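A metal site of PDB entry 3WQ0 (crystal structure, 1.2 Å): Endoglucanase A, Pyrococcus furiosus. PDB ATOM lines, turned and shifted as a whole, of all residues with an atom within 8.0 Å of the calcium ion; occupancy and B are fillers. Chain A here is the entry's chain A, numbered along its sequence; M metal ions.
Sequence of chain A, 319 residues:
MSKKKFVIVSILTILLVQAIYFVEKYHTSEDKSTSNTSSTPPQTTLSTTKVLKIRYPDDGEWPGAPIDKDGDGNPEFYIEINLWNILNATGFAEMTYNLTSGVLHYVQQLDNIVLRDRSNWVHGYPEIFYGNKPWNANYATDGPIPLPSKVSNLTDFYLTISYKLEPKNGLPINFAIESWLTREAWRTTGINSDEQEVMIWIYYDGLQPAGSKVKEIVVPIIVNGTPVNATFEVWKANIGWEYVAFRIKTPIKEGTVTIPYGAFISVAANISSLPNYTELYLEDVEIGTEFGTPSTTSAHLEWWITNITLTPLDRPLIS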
ATOM      1  N   ILE A  67     -18.622   8.032   5.703  1.00  0.00           N
ATOM      2  CA  ILE A  67     -17.714   8.967   5.011  1.00  0.00           C
ATOM      3  C   ILE A  67     -16.394   8.287   4.948  1.00  0.00           C
ATOM      4  O   ILE A  67     -15.756   7.987   5.990  1.00  0.00           O
ATOM      5  CB  ILE A  67     -17.635  10.271   5.811  1.00  0.00           C
ATOM      6  CG1 ILE A  67     -18.995  11.018   5.695  1.00  0.00           C
ATOM      7  CG2 ILE A  67     -16.492  11.141   5.268  1.00  0.00           C
ATOM      8  CD1 ILE A  67     -19.112  12.181   6.630  1.00  0.00           C
ATOM      9  N   ASP A  68     -15.921   7.995   3.741  1.00  0.00           N
ATOM     10  CA  ASP A  68     -14.674   7.218   3.550  1.00  0.00           C
ATOM     11  C   ASP A  68     -13.921   7.900   2.412  1.00  0.00           C
ATOM     12  O   ASP A  68     -13.925   7.436   1.253  1.00  0.00           O
ATOM     13  CB  ASP A  68     -15.009   5.785   3.235  1.00  0.00           C
ATOM     14  CG  ASP A  68     -13.820   4.857   3.096  1.00  0.00           C
ATOM     15  OD1 ASP A  68     -12.719   5.245   3.499  1.00  0.00           O
ATOM     16  OD2 ASP A  68     -14.040   3.723   2.585  1.00  0.00           O
ATOM     17  N   LYS A  69     -13.240   8.984   2.708  1.00  0.00           N
ATOM     18  CA  LYS A  69     -12.706   9.840   1.654  1.00  0.00           C
ATOM     19  C   LYS A  69     -11.591   9.138   0.872  1.00  0.00           C
ATOM     20  O   LYS A  69     -11.391   9.417  -0.283  1.00  0.00           O
ATOM     21  CB  LYS A  69     -12.116  11.116   2.281  1.00  0.00           C
ATOM     22  CG  LYS A  69     -11.523  12.048   1.185  1.00  0.00           C
ATOM     23  CD  LYS A  69     -11.297  13.414   1.729  1.00  0.00           C
ATOM     24  CE  LYS A  69     -10.555  14.291   0.719  1.00  0.00           C
ATOM     25  NZ  LYS A  69     -11.081  14.143  -0.677  1.00  0.00           N
ATOM     26  N   ASP A  70     -10.789   8.285   1.513  1.00  0.00           N
ATOM     27  CA  ASP A  70      -9.724   7.560   0.803  1.00  0.00           C
ATOM     28  C   ASP A  70     -10.217   6.260   0.207  1.00  0.00           C
ATOM     29  O   ASP A  70      -9.423   5.539  -0.370  1.00  0.00           O
ATOM     30  CB  ASP A  70      -8.470   7.405   1.672  1.00  0.00           C
ATOM     31  CG  ASP A  70      -8.686   6.592   2.943  1.00  0.00           C
ATOM     32  OD1 ASP A  70      -9.838   6.357   3.330  1.00  0.00           O
ATOM     33  OD2 ASP A  70      -7.722   6.160   3.607  1.00  0.00           O
ATOM     34  N   GLY A  71     -11.524   5.941   0.376  1.00  0.00           N
ATOM     35  CA  GLY A  71     -12.075   4.707  -0.239  1.00  0.00           C
ATOM     36  C   GLY A  71     -11.411   3.427   0.310  1.00  0.00           C
ATOM     37  O   GLY A  71     -11.335   2.455  -0.450  1.00  0.00           O
ATOM     38  N   ASP A  72     -10.908   3.433   1.560  1.00  0.00           N
ATOM     39  CA  ASP A  72     -10.204   2.297   2.054  1.00  0.00           C
ATOM     40  C   ASP A  72     -11.051   1.341   2.854  1.00  0.00           C
ATOM     41  O   ASP A  72     -10.509   0.353   3.345  1.00  0.00           O
ATOM     42  CB  ASP A  72      -8.927   2.689   2.810  1.00  0.00           C
ATOM     43  CG  ASP A  72      -9.194   3.144   4.234  1.00  0.00           C
ATOM     44  OD1 ASP A  72     -10.351   3.472   4.568  1.00  0.00           O
ATOM     45  OD2 ASP A  72      -8.219   3.198   5.051  1.00  0.00           O
ATOM     46  N   GLY A  73     -12.352   1.503   2.878  1.00  0.00           N
ATOM     47  CA  GLY A  73     -13.239   0.576   3.563  1.00  0.00           C
ATOM     48  C   GLY A  73     -13.328   0.800   5.042  1.00  0.00           C
ATOM     49  O   GLY A  73     -14.041   0.037   5.715  1.00  0.00           O
ATOM     50  N   ASN A  74     -12.639   1.798   5.603  1.00  0.00           N
ATOM     51  CA  ASN A  74     -12.741   2.128   7.033  1.00  0.00           C
ATOM     52  C   ASN A  74     -13.192   3.562   7.058  1.00  0.00           C
ATOM     53  O   ASN A  74     -12.438   4.466   6.717  1.00  0.00           O
ATOM     54  CB  ASN A  74     -11.388   1.963   7.681  1.00  0.00           C
ATOM     55  CG  ASN A  74     -11.500   2.058   9.209  1.00  0.00           C
ATOM     56  OD1 ASN A  74     -12.627   2.184   9.774  1.00  0.00           O
ATOM     57  ND2 ASN A  74     -10.366   2.009   9.871  1.00  0.00           N
ATOM     58  N   PRO A  75     -14.454   3.850   7.453  1.00  0.00           N
ATOM     59  CA  PRO A  75     -14.916   5.237   7.388  1.00  0.00           C
ATOM     60  C   PRO A  75     -14.156   6.099   8.410  1.00  0.00           C
ATOM     61  O   PRO A  75     -13.837   5.645   9.526  1.00  0.00           O
ATOM     62  CB  PRO A  75     -16.416   5.111   7.749  1.00  0.00           C
ATOM     63  CG  PRO A  75     -16.769   3.672   7.430  1.00  0.00           C
ATOM     64  CD  PRO A  75     -15.511   2.914   7.867  1.00  0.00           C
ATOM     65  N   GLU A  76     -13.964   7.361   8.026  1.00  0.00           N
ATOM     66  CA  GLU A  76     -13.494   8.366   8.994  1.00  0.00           C
ATOM     67  C   GLU A  76     -14.611   8.828   9.956  1.00  0.00           C
ATOM     68  O   GLU A  76     -14.324   9.174  11.110  1.00  0.00           O
ATOM     69  CB  GLU A  76     -12.904   9.607   8.299  1.00  0.00           C
ATOM     70  CG  GLU A  76     -11.706   9.275   7.368  1.00  0.00           C
ATOM     71  CD  GLU A  76     -12.205   8.872   5.970  1.00  0.00           C
ATOM     72  OE1 GLU A  76     -12.913   9.641   5.311  1.00  0.00           O
ATOM     73  OE2 GLU A  76     -11.847   7.789   5.471  1.00  0.00           O
ATOM     74  N   PHE A  77     -15.837   8.867   9.401  1.00  0.00           N
ATOM     75  CA  PHE A  77     -17.009   9.275  10.184  1.00  0.00           C
ATOM     76  C   PHE A  77     -18.179   8.501   9.603  1.00  0.00           C
ATOM     77  O   PHE A  77     -18.088   7.980   8.481  1.00  0.00           O
ATOM     78  CB  PHE A  77     -17.281  10.778  10.112  1.00  0.00           C
ATOM     79  CG  PHE A  77     -16.260  11.601  10.779  1.00  0.00           C
ATOM     80  CD1 PHE A  77     -16.242  11.784  12.156  1.00  0.00           C
ATOM     81  CD2 PHE A  77     -15.203  12.174  10.059  1.00  0.00           C
ATOM     82  CE1 PHE A  77     -15.217  12.505  12.799  1.00  0.00           C
ATOM     83  CE2 PHE A  77     -14.216  12.908  10.657  1.00  0.00           C
ATOM     84  CZ  PHE A  77     -14.210  13.067  12.028  1.00  0.00           C
ATOM     85  N   THR A 141     -13.741   4.034  12.067  1.00  0.00           N
ATOM     86  CA  THR A 141     -12.540   3.895  12.910  1.00  0.00           C
ATOM     87  C   THR A 141     -11.293   4.367  12.254  1.00  0.00           C
ATOM     88  O   THR A 141     -10.182   4.166  12.779  1.00  0.00           O
ATOM     89  CB  THR A 141     -12.383   2.469  13.455  1.00  0.00           C
ATOM     90  OG1 THR A 141     -12.079   1.589  12.415  1.00  0.00           O
ATOM     91  CG2 THR A 141     -13.608   2.013  14.249  1.00  0.00           C
ATOM     92  N   ASP A 142     -11.411   5.168  11.187  1.00  0.00           N
ATOM     93  CA  ASP A 142     -10.215   5.720  10.504  1.00  0.00           C
ATOM     94  C   ASP A 142      -9.933   7.060  11.074  1.00  0.00           C
ATOM     95  O   ASP A 142     -10.423   8.085  10.585  1.00  0.00           O
ATOM     96  CB  ASP A 142     -10.506   5.732   9.013  1.00  0.00           C
ATOM     97  CG  ASP A 142      -9.307   6.075   8.096  1.00  0.00           C
ATOM     98  OD1 ASP A 142      -8.261   6.473   8.656  1.00  0.00           O
ATOM     99  OD2 ASP A 142      -9.463   5.963   6.822  1.00  0.00           O
ATOM    100  N   GLY A 143      -9.229   7.112  12.197  1.00  0.00           N
ATOM    101  CA  GLY A 143      -8.931   8.374  12.870  1.00  0.00           C
ATOM    102  C   GLY A 143      -7.862   8.119  13.922  1.00  0.00           C
ATOM    103  O   GLY A 143      -7.481   6.942  14.178  1.00  0.00           O
HETATM  104 CA    CA M   1     -11.089   5.634   5.185  1.00  0.00          CA
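The side-chain carboxylate of Asp 68 sits close to the backbone NH of Gly 71 (3.4 Å). The side-chain amide oxygen (OD1) of Asn 74 is in hydrogen-bond range of the side-chain hydroxyl (OG1) of Thr 141 (2.8 Å). The backbone NH of Lys 69 lies within hydrogen-bond range of the side-chain carboxylate of Glu 76 (2.7 Å). N of Gly 73 is in hydrogen-bond range of OD2 of Asp 68, at 2.8 Å. The backbone carbonyl oxygen (O) of Pro 75 is in hydrogen-bond range of the backbone NH (N) of Asp 142 (3.0 Å). The backbone carbonyl oxygen (O) of Ile 67 is in hydrogen-bond range of the backbone NH (N) of Glu 76, 2.8 Å away.
Within 4 Å of the calcium ion: Asp 68, Asp 70, Asp 72, Asn 74, Glu 76 and Asp 142.
The calcium ion is bound by the side-chain carboxylate (OE2) of Glu 76 (2.3 Å), the side-chain carboxylate (OD2) of Asp 142 (2.3 Å), the side-chain carboxylate (OD1) of Asp 70 (2.4 Å), the backbone carbonyl oxygen (O) of Asn 74 (2.4 Å), the side-chain carboxylate (OD1) of Asp 72 (2.4 Å) and the side-chain carboxylate (OD1) of Asp 68 (2.4 Å). The calcium ion has six donor atoms within binding distance.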
